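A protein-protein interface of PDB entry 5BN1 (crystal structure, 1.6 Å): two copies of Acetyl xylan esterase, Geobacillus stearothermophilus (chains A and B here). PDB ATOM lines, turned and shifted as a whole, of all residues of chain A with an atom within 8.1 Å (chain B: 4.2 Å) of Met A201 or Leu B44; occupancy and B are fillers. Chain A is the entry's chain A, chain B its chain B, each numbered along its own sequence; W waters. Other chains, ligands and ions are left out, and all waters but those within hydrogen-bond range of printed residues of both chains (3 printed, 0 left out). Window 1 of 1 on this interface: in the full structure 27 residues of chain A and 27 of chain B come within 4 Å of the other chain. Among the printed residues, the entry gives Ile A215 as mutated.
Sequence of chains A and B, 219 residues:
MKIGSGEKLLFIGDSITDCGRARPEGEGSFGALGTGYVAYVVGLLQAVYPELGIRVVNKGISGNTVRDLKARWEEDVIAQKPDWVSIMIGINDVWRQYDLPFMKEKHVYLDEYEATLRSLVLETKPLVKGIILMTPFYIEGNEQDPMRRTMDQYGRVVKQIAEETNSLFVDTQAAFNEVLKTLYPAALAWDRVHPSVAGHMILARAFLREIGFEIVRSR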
ATOM      1  N   THR A  35     -15.167 -24.617 -33.830  1.00  0.00           N
ATOM      2  CA  THR A  35     -14.835 -23.779 -32.677  1.00  0.00           C
ATOM      3  C   THR A  35     -14.888 -24.417 -31.327  1.00  0.00           C
ATOM      4  O   THR A  35     -15.168 -23.761 -30.309  1.00  0.00           O
ATOM      5  CB  THR A  35     -15.779 -22.530 -32.641  1.00  0.00           C
ATOM      6  OG1 THR A  35     -17.138 -22.964 -32.664  1.00  0.00           O
ATOM      7  CG2 THR A  35     -15.485 -21.706 -33.914  1.00  0.00           C
ATOM      8  N   GLY A  36     -14.578 -25.711 -31.216  1.00  0.00           N
ATOM      9  CA  GLY A  36     -14.672 -26.439 -29.963  1.00  0.00           C
ATOM     10  C   GLY A  36     -13.390 -27.254 -29.789  1.00  0.00           C
ATOM     11  O   GLY A  36     -12.250 -26.903 -30.116  1.00  0.00           O
ATOM     12  N   TYR A  37     -13.616 -28.405 -29.142  1.00  0.00           N
ATOM     13  CA  TYR A  37     -12.462 -29.124 -28.550  1.00  0.00           C
ATOM     14  C   TYR A  37     -11.471 -29.580 -29.653  1.00  0.00           C
ATOM     15  O   TYR A  37     -10.296 -29.609 -29.338  1.00  0.00           O
ATOM     16  CB  TYR A  37     -12.836 -30.339 -27.658  1.00  0.00           C
ATOM     17  CG  TYR A  37     -13.281 -31.608 -28.351  1.00  0.00           C
ATOM     18  CD1 TYR A  37     -14.580 -31.820 -28.816  1.00  0.00           C
ATOM     19  CD2 TYR A  37     -12.327 -32.580 -28.690  1.00  0.00           C
ATOM     20  CE1 TYR A  37     -14.968 -32.960 -29.528  1.00  0.00           C
ATOM     21  CE2 TYR A  37     -12.724 -33.705 -29.388  1.00  0.00           C
ATOM     22  CZ  TYR A  37     -13.985 -33.894 -29.809  1.00  0.00           C
ATOM     23  OH  TYR A  37     -14.386 -35.028 -30.574  1.00  0.00           O
ATOM     24  N   ALA A  39     -10.581 -27.985 -32.377  1.00  0.00           N
ATOM     25  CA  ALA A  39      -9.724 -26.869 -32.649  1.00  0.00           C
ATOM     26  C   ALA A  39      -8.804 -26.600 -31.500  1.00  0.00           C
ATOM     27  O   ALA A  39      -7.650 -26.161 -31.733  1.00  0.00           O
ATOM     28  CB  ALA A  39     -10.560 -25.634 -32.971  1.00  0.00           C
ATOM     29  N   TYR A  40      -9.287 -26.690 -30.276  1.00  0.00           N
ATOM     30  CA  TYR A  40      -8.481 -26.431 -29.116  1.00  0.00           C
ATOM     31  C   TYR A  40      -7.309 -27.409 -28.977  1.00  0.00           C
ATOM     32  O   TYR A  40      -6.194 -27.061 -28.614  1.00  0.00           O
ATOM     33  CB  TYR A  40      -9.275 -26.361 -27.826  1.00  0.00           C
ATOM     34  CG  TYR A  40     -10.380 -25.348 -27.749  1.00  0.00           C
ATOM     35  CD1 TYR A  40     -10.430 -24.328 -28.634  1.00  0.00           C
ATOM     36  CD2 TYR A  40     -11.245 -25.391 -26.751  1.00  0.00           C
ATOM     37  CE1 TYR A  40     -11.501 -23.398 -28.582  1.00  0.00           C
ATOM     38  CE2 TYR A  40     -12.339 -24.502 -26.672  1.00  0.00           C
ATOM     39  CZ  TYR A  40     -12.421 -23.526 -27.564  1.00  0.00           C
ATOM     40  OH  TYR A  40     -13.463 -22.552 -27.485  1.00  0.00           O
ATOM     41  N   VAL A  41      -7.608 -28.696 -29.264  1.00  0.00           N
ATOM     42  CA  VAL A  41      -6.560 -29.683 -29.290  1.00  0.00           C
ATOM     43  C   VAL A  41      -5.479 -29.308 -30.300  1.00  0.00           C
ATOM     44  O   VAL A  41      -4.286 -29.354 -29.963  1.00  0.00           O
ATOM     45  CB  VAL A  41      -7.200 -31.090 -29.573  1.00  0.00           C
ATOM     46  CG1 VAL A  41      -6.112 -32.062 -30.039  1.00  0.00           C
ATOM     47  CG2 VAL A  41      -8.014 -31.640 -28.391  1.00  0.00           C
ATOM     48  N   LEU A  44      -3.525 -26.093 -29.059  1.00  0.00           N
ATOM     49  CA  LEU A  44      -2.654 -26.367 -27.959  1.00  0.00           C
ATOM     50  C   LEU A  44      -1.389 -27.177 -28.437  1.00  0.00           C
ATOM     51  O   LEU A  44      -0.269 -26.920 -28.007  1.00  0.00           O
ATOM     52  CB  LEU A  44      -3.349 -27.099 -26.831  1.00  0.00           C
ATOM     53  CG  LEU A  44      -4.235 -26.160 -25.934  1.00  0.00           C
ATOM     54  CD1 LEU A  44      -5.256 -26.923 -25.192  1.00  0.00           C
ATOM     55  CD2 LEU A  44      -3.250 -25.389 -25.001  1.00  0.00           C
ATOM     56  N   ALA A 175     -14.053 -36.610 -16.701  1.00  0.00           N
ATOM     57  CA  ALA A 175     -13.435 -35.243 -16.826  1.00  0.00           C
ATOM     58  C   ALA A 175     -14.477 -34.206 -16.366  1.00  0.00           C
ATOM     59  O   ALA A 175     -14.191 -33.302 -15.559  1.00  0.00           O
ATOM     60  CB  ALA A 175     -12.963 -35.020 -18.198  1.00  0.00           C
ATOM     61  N   PHE A 176     -15.727 -34.372 -16.818  1.00  0.00           N
ATOM     62  CA  PHE A 176     -16.776 -33.435 -16.341  1.00  0.00           C
ATOM     63  C   PHE A 176     -17.118 -33.619 -14.876  1.00  0.00           C
ATOM     64  O   PHE A 176     -17.410 -32.718 -14.155  1.00  0.00           O
ATOM     65  CB  PHE A 176     -18.012 -33.524 -17.186  1.00  0.00           C
ATOM     66  CG  PHE A 176     -17.907 -32.793 -18.506  1.00  0.00           C
ATOM     67  CD1 PHE A 176     -17.931 -31.371 -18.489  1.00  0.00           C
ATOM     68  CD2 PHE A 176     -17.827 -33.438 -19.686  1.00  0.00           C
ATOM     69  CE1 PHE A 176     -17.819 -30.724 -19.663  1.00  0.00           C
ATOM     70  CE2 PHE A 176     -17.733 -32.784 -20.871  1.00  0.00           C
ATOM     71  CZ  PHE A 176     -17.647 -31.365 -20.837  1.00  0.00           C
ATOM     72  N   LEU A 188     -21.807 -24.748 -17.124  1.00  0.00           N
ATOM     73  CA  LEU A 188     -21.094 -25.273 -18.251  1.00  0.00           C
ATOM     74  C   LEU A 188     -21.981 -25.460 -19.495  1.00  0.00           C
ATOM     75  O   LEU A 188     -21.502 -25.319 -20.642  1.00  0.00           O
ATOM     76  CB  LEU A 188     -20.500 -26.646 -17.901  1.00  0.00           C
ATOM     77  CG  LEU A 188     -19.374 -26.611 -16.839  1.00  0.00           C
ATOM     78  CD1 LEU A 188     -19.140 -28.066 -16.384  1.00  0.00           C
ATOM     79  CD2 LEU A 188     -18.147 -26.010 -17.468  1.00  0.00           C
ATOM     80  N   PRO A 195     -21.493 -27.474 -24.376  1.00  0.00           N
ATOM     81  CA  PRO A 195     -20.870 -26.650 -23.381  1.00  0.00           C
ATOM     82  C   PRO A 195     -20.228 -25.342 -23.888  1.00  0.00           C
ATOM     83  O   PRO A 195     -20.095 -25.144 -25.082  1.00  0.00           O
ATOM     84  CB  PRO A 195     -19.816 -27.540 -22.746  1.00  0.00           C
ATOM     85  CG  PRO A 195     -19.373 -28.270 -23.851  1.00  0.00           C
ATOM     86  CD  PRO A 195     -20.535 -28.500 -24.837  1.00  0.00           C
ATOM     87  N   SER A 196     -19.943 -24.531 -22.898  1.00  0.00           N
ATOM     88  CA  SER A 196     -19.171 -23.310 -23.111  1.00  0.00           C
ATOM     89  C   SER A 196     -17.753 -23.653 -23.579  1.00  0.00           C
ATOM     90  O   SER A 196     -17.271 -24.838 -23.615  1.00  0.00           O
ATOM     91  CB  SER A 196     -18.921 -22.550 -21.820  1.00  0.00           C
ATOM     92  OG  SER A 196     -18.331 -23.297 -20.818  1.00  0.00           O
ATOM     93  N   VAL A 197     -16.957 -22.613 -23.833  1.00  0.00           N
ATOM     94  CA  VAL A 197     -15.534 -22.786 -24.094  1.00  0.00           C
ATOM     95  C   VAL A 197     -14.908 -23.619 -23.009  1.00  0.00           C
ATOM     96  O   VAL A 197     -13.993 -24.444 -23.219  1.00  0.00           O
ATOM     97  CB  VAL A 197     -14.804 -21.409 -24.176  1.00  0.00           C
ATOM     98  CG1 VAL A 197     -13.276 -21.558 -24.158  1.00  0.00           C
ATOM     99  CG2 VAL A 197     -15.357 -20.612 -25.352  1.00  0.00           C
ATOM    100  N   ALA A 198     -15.220 -23.395 -21.742  1.00  0.00           N
ATOM    101  CA  ALA A 198     -14.663 -24.137 -20.638  1.00  0.00           C
ATOM    102  C   ALA A 198     -14.937 -25.645 -20.786  1.00  0.00           C
ATOM    103  O   ALA A 198     -14.020 -26.436 -20.529  1.00  0.00           O
ATOM    104  CB  ALA A 198     -15.224 -23.679 -19.307  1.00  0.00           C
ATOM    105  N   GLY A 199     -16.129 -26.008 -21.157  1.00  0.00           N
ATOM    106  CA  GLY A 199     -16.432 -27.413 -21.402  1.00  0.00           C
ATOM    107  C   GLY A 199     -15.657 -28.005 -22.498  1.00  0.00           C
ATOM    108  O   GLY A 199     -15.173 -29.169 -22.389  1.00  0.00           O
ATOM    109  N   HIS A 200     -15.449 -27.247 -23.570  1.00  0.00           N
ATOM    110  CA  HIS A 200     -14.601 -27.716 -24.693  1.00  0.00           C
ATOM    111  C   HIS A 200     -13.172 -27.837 -24.223  1.00  0.00           C
ATOM    112  O   HIS A 200     -12.413 -28.695 -24.735  1.00  0.00           O
ATOM    113  CB  HIS A 200     -14.814 -26.880 -25.929  1.00  0.00           C
ATOM    114  CG  HIS A 200     -16.019 -27.337 -26.701  1.00  0.00           C
ATOM    115  ND1 HIS A 200     -17.314 -26.825 -26.635  1.00  0.00           N
ATOM    116  CD2 HIS A 200     -16.112 -28.378 -27.503  1.00  0.00           C
ATOM    117  CE1 HIS A 200     -18.114 -27.542 -27.444  1.00  0.00           C
ATOM    118  NE2 HIS A 200     -17.349 -28.495 -27.982  1.00  0.00           N
ATOM    119  N   MET A 201     -12.715 -26.959 -23.324  1.00  0.00           N
ATOM    120  CA  MET A 201     -11.398 -27.069 -22.754  1.00  0.00           C
ATOM    121  C   MET A 201     -11.262 -28.321 -21.926  1.00  0.00           C
ATOM    122  O   MET A 201     -10.223 -28.977 -21.941  1.00  0.00           O
ATOM    123  CB  MET A 201     -10.989 -25.858 -21.884  1.00  0.00           C
ATOM    124  CG  MET A 201     -10.687 -24.696 -22.779  1.00  0.00           C
ATOM    125  SD  MET A 201      -9.134 -24.883 -23.768  1.00  0.00           S
ATOM    126  CE  MET A 201      -9.375 -23.214 -24.432  1.00  0.00           C
ATOM    127  N   ILE A 202     -12.266 -28.631 -21.136  1.00  0.00           N
ATOM    128  CA  ILE A 202     -12.307 -29.933 -20.344  1.00  0.00           C
ATOM    129  C   ILE A 202     -12.085 -31.086 -21.308  1.00  0.00           C
ATOM    130  O   ILE A 202     -11.263 -31.991 -21.031  1.00  0.00           O
ATOM    131  CB  ILE A 202     -13.597 -30.022 -19.546  1.00  0.00           C
ATOM    132  CG1 ILE A 202     -13.646 -29.029 -18.406  1.00  0.00           C
ATOM    133  CG2 ILE A 202     -13.799 -31.477 -19.024  1.00  0.00           C
ATOM    134  CD1 ILE A 202     -15.049 -28.832 -17.844  1.00  0.00           C
ATOM    135  N   LEU A 203     -12.828 -31.108 -22.378  1.00  0.00           N
ATOM    136  CA  LEU A 203     -12.708 -32.148 -23.409  1.00  0.00           C
ATOM    137  C   LEU A 203     -11.334 -32.175 -24.008  1.00  0.00           C
ATOM    138  O   LEU A 203     -10.722 -33.226 -24.155  1.00  0.00           O
ATOM    139  CB  LEU A 203     -13.751 -32.052 -24.473  1.00  0.00           C
ATOM    140  CG  LEU A 203     -15.208 -32.272 -24.059  1.00  0.00           C
ATOM    141  CD1 LEU A 203     -16.175 -31.820 -25.132  1.00  0.00           C
ATOM    142  CD2 LEU A 203     -15.383 -33.792 -23.839  1.00  0.00           C
ATOM    143  N   ALA A 204     -10.816 -31.005 -24.438  1.00  0.00           N
ATOM    144  CA  ALA A 204      -9.482 -30.999 -25.085  1.00  0.00           C
ATOM    145  C   ALA A 204      -8.445 -31.493 -24.084  1.00  0.00           C
ATOM    146  O   ALA A 204      -7.495 -32.240 -24.469  1.00  0.00           O
ATOM    147  CB  ALA A 204      -9.161 -29.606 -25.529  1.00  0.00           C
ATOM    148  N   ARG A 205      -8.501 -31.077 -22.833  1.00  0.00           N
ATOM    149  CA  ARG A 205      -7.547 -31.467 -21.840  1.00  0.00           C
ATOM    150  C   ARG A 205      -7.601 -33.011 -21.622  1.00  0.00           C
ATOM    151  O   ARG A 205      -6.544 -33.641 -21.564  1.00  0.00           O
ATOM    152  CB  ARG A 205      -7.888 -30.760 -20.537  1.00  0.00           C
ATOM    153  CG  ARG A 205      -6.995 -31.159 -19.416  1.00  0.00           C
ATOM    154  CD  ARG A 205      -7.368 -30.489 -18.107  1.00  0.00           C
ATOM    155  NE  ARG A 205      -6.385 -30.746 -17.061  1.00  0.00           N
ATOM    156  CZ  ARG A 205      -6.681 -30.895 -15.781  1.00  0.00           C
ATOM    157  NH1 ARG A 205      -7.886 -30.738 -15.345  1.00  0.00           N
ATOM    158  NH2 ARG A 205      -5.699 -31.143 -14.890  1.00  0.00           N
ATOM    159  N   ALA A 206      -8.806 -33.550 -21.634  1.00  0.00           N
ATOM    160  CA  ALA A 206      -8.896 -35.056 -21.480  1.00  0.00           C
ATOM    161  C   ALA A 206      -8.357 -35.746 -22.662  1.00  0.00           C
ATOM    162  O   ALA A 206      -7.628 -36.819 -22.478  1.00  0.00           O
ATOM    163  CB  ALA A 206     -10.331 -35.417 -21.198  1.00  0.00           C
ATOM    164  N   PHE A 207      -8.598 -35.314 -23.872  1.00  0.00           N
ATOM    165  CA  PHE A 207      -8.043 -35.877 -25.096  1.00  0.00           C
ATOM    166  C   PHE A 207      -6.521 -35.826 -25.032  1.00  0.00           C
ATOM    167  O   PHE A 207      -5.825 -36.850 -25.294  1.00  0.00           O
ATOM    168  CB  PHE A 207      -8.615 -35.260 -26.304  1.00  0.00           C
ATOM    169  CG  PHE A 207      -8.077 -35.834 -27.555  1.00  0.00           C
ATOM    170  CD1 PHE A 207      -6.908 -35.362 -28.135  1.00  0.00           C
ATOM    171  CD2 PHE A 207      -8.755 -36.891 -28.175  1.00  0.00           C
ATOM    172  CE1 PHE A 207      -6.408 -35.929 -29.284  1.00  0.00           C
ATOM    173  CE2 PHE A 207      -8.254 -37.446 -29.331  1.00  0.00           C
ATOM    174  CZ  PHE A 207      -7.084 -36.953 -29.886  1.00  0.00           C
ATOM    175  N   LEU A 208      -6.006 -34.612 -24.792  1.00  0.00           N
ATOM    176  CA  LEU A 208      -4.579 -34.434 -24.792  1.00  0.00           C
ATOM    177  C   LEU A 208      -3.864 -35.324 -23.796  1.00  0.00           C
ATOM    178  O   LEU A 208      -2.767 -35.900 -24.133  1.00  0.00           O
ATOM    179  CB  LEU A 208      -4.251 -32.931 -24.579  1.00  0.00           C
ATOM    180  CG  LEU A 208      -4.554 -32.023 -25.768  1.00  0.00           C
ATOM    181  CD1 LEU A 208      -4.574 -30.570 -25.389  1.00  0.00           C
ATOM    182  CD2 LEU A 208      -3.612 -32.224 -26.954  1.00  0.00           C
ATOM    183  N   ILE A 215      -1.972 -31.553 -19.145  1.00  0.00           N
ATOM    184  CA  ILE A 215      -2.003 -30.196 -18.568  1.00  0.00           C
ATOM    185  C   ILE A 215      -2.437 -30.360 -17.106  1.00  0.00           C
ATOM    186  O   ILE A 215      -3.513 -30.925 -16.779  1.00  0.00           O
ATOM    187  CB  ILE A 215      -2.993 -29.353 -19.352  1.00  0.00           C
ATOM    188  CG1 ILE A 215      -2.521 -29.280 -20.771  1.00  0.00           C
ATOM    189  CG2 ILE A 215      -3.376 -28.084 -18.552  1.00  0.00           C
ATOM    190  CD1 ILE A 215      -3.478 -28.606 -21.724  1.00  0.00           C
ATOM    191  N   TYR B  40      -9.911 -18.086 -24.057  1.00  0.00           N
ATOM    192  CA  TYR B  40      -9.080 -19.273 -23.739  1.00  0.00           C
ATOM    193  C   TYR B  40      -8.532 -19.324 -22.365  1.00  0.00           C
ATOM    194  O   TYR B  40      -8.519 -20.305 -21.645  1.00  0.00           O
ATOM    195  CB  TYR B  40      -8.009 -19.516 -24.797  1.00  0.00           C
ATOM    196  CG  TYR B  40      -8.454 -19.662 -26.174  1.00  0.00           C
ATOM    197  CD1 TYR B  40      -9.749 -19.925 -26.509  1.00  0.00           C
ATOM    198  CD2 TYR B  40      -7.587 -19.600 -27.239  1.00  0.00           C
ATOM    199  CE1 TYR B  40     -10.223 -20.048 -27.822  1.00  0.00           C
ATOM    200  CE2 TYR B  40      -8.003 -19.734 -28.554  1.00  0.00           C
ATOM    201  CZ  TYR B  40      -9.303 -19.920 -28.841  1.00  0.00           C
ATOM    202  OH  TYR B  40      -9.684 -20.027 -30.156  1.00  0.00           O
ATOM    203  N   VAL B  41      -8.038 -18.166 -21.908  1.00  0.00           N
ATOM    204  CA  VAL B  41      -7.559 -18.017 -20.563  1.00  0.00           C
ATOM    205  C   VAL B  41      -8.709 -18.373 -19.544  1.00  0.00           C
ATOM    206  O   VAL B  41      -8.488 -19.153 -18.604  1.00  0.00           O
ATOM    207  CB  VAL B  41      -7.082 -16.533 -20.322  1.00  0.00           C
ATOM    208  CG1 VAL B  41      -6.950 -16.300 -18.836  1.00  0.00           C
ATOM    209  CG2 VAL B  41      -5.764 -16.316 -21.007  1.00  0.00           C
ATOM    210  N   VAL B  42      -9.882 -17.811 -19.766  1.00  0.00           N
ATOM    211  CA  VAL B  42     -11.038 -18.040 -18.859  1.00  0.00           C
ATOM    212  C   VAL B  42     -11.415 -19.542 -18.929  1.00  0.00           C
ATOM    213  O   VAL B  42     -11.608 -20.146 -17.867  1.00  0.00           O
ATOM    214  CB  VAL B  42     -12.196 -17.124 -19.145  1.00  0.00           C
ATOM    215  CG1 VAL B  42     -13.437 -17.438 -18.246  1.00  0.00           C
ATOM    216  CG2 VAL B  42     -11.706 -15.664 -18.961  1.00  0.00           C
ATOM    217  N   GLY B  43     -11.419 -20.093 -20.142  1.00  0.00           N
ATOM    218  CA  GLY B  43     -11.803 -21.500 -20.243  1.00  0.00           C
ATOM    219  C   GLY B  43     -10.860 -22.442 -19.594  1.00  0.00           C
ATOM    220  O   GLY B  43     -11.240 -23.453 -18.933  1.00  0.00           O
ATOM    221  N   LEU B  44      -9.565 -22.221 -19.789  1.00  0.00           N
ATOM    222  CA  LEU B  44      -8.530 -23.044 -19.154  1.00  0.00           C
ATOM    223  C   LEU B  44      -8.553 -22.921 -17.666  1.00  0.00           C
ATOM    224  O   LEU B  44      -8.414 -23.922 -16.932  1.00  0.00           O
ATOM    225  CB  LEU B  44      -7.157 -22.739 -19.708  1.00  0.00           C
ATOM    226  CG  LEU B  44      -6.878 -23.274 -21.136  1.00  0.00           C
ATOM    227  CD1 LEU B  44      -5.773 -22.526 -21.821  1.00  0.00           C
ATOM    228  CD2 LEU B  44      -6.518 -24.778 -21.002  1.00  0.00           C
ATOM    229  N   LEU B  45      -8.733 -21.701 -17.146  1.00  0.00           N
ATOM    230  CA  LEU B  45      -8.866 -21.560 -15.711  1.00  0.00           C
ATOM    231  C   LEU B  45     -10.123 -22.279 -15.171  1.00  0.00           C
ATOM    232  O   LEU B  45     -10.045 -22.852 -14.046  1.00  0.00           O
ATOM    233  CB  LEU B  45      -8.913 -20.075 -15.327  1.00  0.00           C
ATOM    234  CG  LEU B  45      -7.534 -19.395 -15.431  1.00  0.00           C
ATOM    235  CD1 LEU B  45      -7.748 -17.918 -15.318  1.00  0.00           C
ATOM    236  CD2 LEU B  45      -6.536 -19.858 -14.403  1.00  0.00           C
ATOM    237  N   GLN B  46     -11.238 -22.191 -15.860  1.00  0.00           N
ATOM    238  CA  GLN B  46     -12.450 -22.884 -15.376  1.00  0.00           C
ATOM    239  C   GLN B  46     -12.261 -24.379 -15.450  1.00  0.00           C
ATOM    240  O   GLN B  46     -12.692 -25.142 -14.514  1.00  0.00           O
ATOM    241  CB  GLN B  46     -13.647 -22.415 -16.101  1.00  0.00           C
ATOM    242  CG  GLN B  46     -14.891 -23.044 -15.465  1.00  0.00           C
ATOM    243  CD  GLN B  46     -16.084 -22.137 -15.707  1.00  0.00           C
ATOM    244  OE1 GLN B  46     -16.485 -21.871 -16.875  1.00  0.00           O
ATOM    245  NE2 GLN B  46     -16.534 -21.487 -14.601  1.00  0.00           N
ATOM    246  N   ALA B  47     -11.644 -24.887 -16.517  1.00  0.00           N
ATOM    247  CA  ALA B  47     -11.429 -26.337 -16.660  1.00  0.00           C
ATOM    248  C   ALA B  47     -10.511 -26.909 -15.605  1.00  0.00           C
ATOM    249  O   ALA B  47     -10.749 -28.018 -15.088  1.00  0.00           O
ATOM    250  CB  ALA B  47     -10.877 -26.623 -17.998  1.00  0.00           C
ATOM    251  N   VAL B  48      -9.448 -26.178 -15.197  1.00  0.00           N
ATOM    252  CA  VAL B  48      -8.421 -26.706 -14.378  1.00  0.00           C
ATOM    253  C   VAL B  48      -8.526 -26.194 -12.918  1.00  0.00           C
ATOM    254  O   VAL B  48      -8.233 -26.943 -12.011  1.00  0.00           O
ATOM    255  CB  VAL B  48      -7.028 -26.421 -14.932  1.00  0.00           C
ATOM    256  CG1 VAL B  48      -5.877 -26.898 -14.092  1.00  0.00           C
ATOM    257  CG2 VAL B  48      -6.831 -26.955 -16.317  1.00  0.00           C
ATOM    258  N   MET B 201      -3.719 -19.469 -28.525  1.00  0.00           N
ATOM    259  CA  MET B 201      -3.267 -20.315 -27.518  1.00  0.00           C
ATOM    260  C   MET B 201      -1.830 -20.030 -26.975  1.00  0.00           C
ATOM    261  O   MET B 201      -1.565 -20.137 -25.772  1.00  0.00           O
ATOM    262  CB  MET B 201      -3.336 -21.844 -27.953  1.00  0.00           C
ATOM    263  CG  MET B 201      -4.667 -22.404 -28.141  1.00  0.00           C
ATOM    264  SD  MET B 201      -5.503 -22.553 -26.470  1.00  0.00           S
ATOM    265  CE  MET B 201      -6.957 -23.272 -27.216  1.00  0.00           C
ATOM    266  N   LEU B 208      -1.069 -17.047 -18.868  1.00  0.00           N
ATOM    267  CA  LEU B 208      -1.307 -17.911 -17.723  1.00  0.00           C
ATOM    268  C   LEU B 208      -0.046 -18.192 -16.939  1.00  0.00           C
ATOM    269  O   LEU B 208      -0.052 -18.234 -15.715  1.00  0.00           O
ATOM    270  CB  LEU B 208      -1.897 -19.253 -18.186  1.00  0.00           C
ATOM    271  CG  LEU B 208      -3.361 -19.099 -18.574  1.00  0.00           C
ATOM    272  CD1 LEU B 208      -3.874 -20.325 -19.329  1.00  0.00           C
ATOM    273  CD2 LEU B 208      -4.294 -18.828 -17.373  1.00  0.00           C
ATOM    274  N   PHE B 213       0.004 -20.159 -13.622  1.00  0.00           N
ATOM    275  CA  PHE B 213      -0.469 -21.420 -14.210  1.00  0.00           C
ATOM    276  C   PHE B 213       0.393 -21.725 -15.422  1.00  0.00           C
ATOM    277  O   PHE B 213       0.099 -21.264 -16.521  1.00  0.00           O
ATOM    278  CB  PHE B 213      -1.925 -21.338 -14.596  1.00  0.00           C
ATOM    279  CG  PHE B 213      -2.501 -22.571 -15.293  1.00  0.00           C
ATOM    280  CD1 PHE B 213      -1.835 -23.830 -15.251  1.00  0.00           C
ATOM    281  CD2 PHE B 213      -3.767 -22.505 -15.908  1.00  0.00           C
ATOM    282  CE1 PHE B 213      -2.379 -24.902 -15.917  1.00  0.00           C
ATOM    283  CE2 PHE B 213      -4.293 -23.630 -16.562  1.00  0.00           C
ATOM    284  CZ  PHE B 213      -3.557 -24.804 -16.562  1.00  0.00           C
HETATM  285  O   HOH W   1     -18.543 -22.337 -18.456  1.00  0.00           O
HETATM  286  O   HOH W   2      -7.848 -29.712 -12.317  1.00  0.00           O
HETATM  287  O   HOH W   3     -10.527 -30.303 -16.576  1.00  0.00           O
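Tyr A40 touches Tyr B40 (CE1 to CE1, 3.7 Å).
Gln B46 touches Ala A198.
Met A201 touches Tyr B40.
Gly B43 touches Met A201.
Met A201 touches Leu B44.
Met B201 touches Met A201.
Ala B47 touches Ile A202 (CB to CG1, 3.7 Å).
Arg A205 touches Ala B47.
CG2 of Val B48 touches NE of Arg A205 (3.9 Å).
Ile A215 touches Phe B213.
Water W1 bridges the side-chain hydroxyl of Ser A196 and the side-chain amide oxygen of Gln B46.
Water W3 bridges the backbone carbonyl oxygen (O) of Ala B47 and the guanidinium group (NH1) of Arg A205.
Water W2 lies within hydrogen-bond range of the backbone carbonyl oxygen (O) of Val B48 (2.8 Å) and the guanidinium group (NH1) of Arg A205 (3.2 Å).
Of the printed residues of chain B, Tyr A40 touches Tyr B40 and Met B201.
Printed residues of chain B within 4 Å of Met A201: Tyr B40 (3.9 Å), Gly B43 (3.8 Å), Leu B44 (3.8 Å), Ala B47 (3.96 Å) and Met B201 (3.7 Å).
Printed residues of chain A within 4 Å of Tyr B40: Tyr A40 and Met A201.
Gly B43 touches just these residues of chain A: Ala A198 and Met A201.
Leu B44 touches just one residue of chain A: Met A201 (3.8 Å).
Tyr A40 touches its own counterpart, Tyr B40.
Tyr A40 touches Met B201, and with the chains exchanged Met A201 touches Tyr B40.
Leu A44 touches Met B201, and with the chains exchanged Met A201 touches Leu B44.
Met B201 touches its own counterpart, Met A201.
The guanidinium group (NE) of Arg A205 lies within hydrogen-bond range of the backbone carbonyl oxygen (O) of Ile A215, at 2.9 Å.
OG of Ser A196 sits close to N of Ala A198 (3.2 Å).
O of Leu B208 lies within hydrogen-bond range of N of Phe B213, 2.8 Å away.
Of the 25 printed residues of chain A, 7 touch a printed residue of chain B.
Hydrophobic or aromatic side chains of chain A within 4 Å of the printed part of chain B: Tyr A40, Leu A44, Ala A198, Met A201, Ile A202 and Ile A215.
Among the printed residues, 14 pairs touch across the chains.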
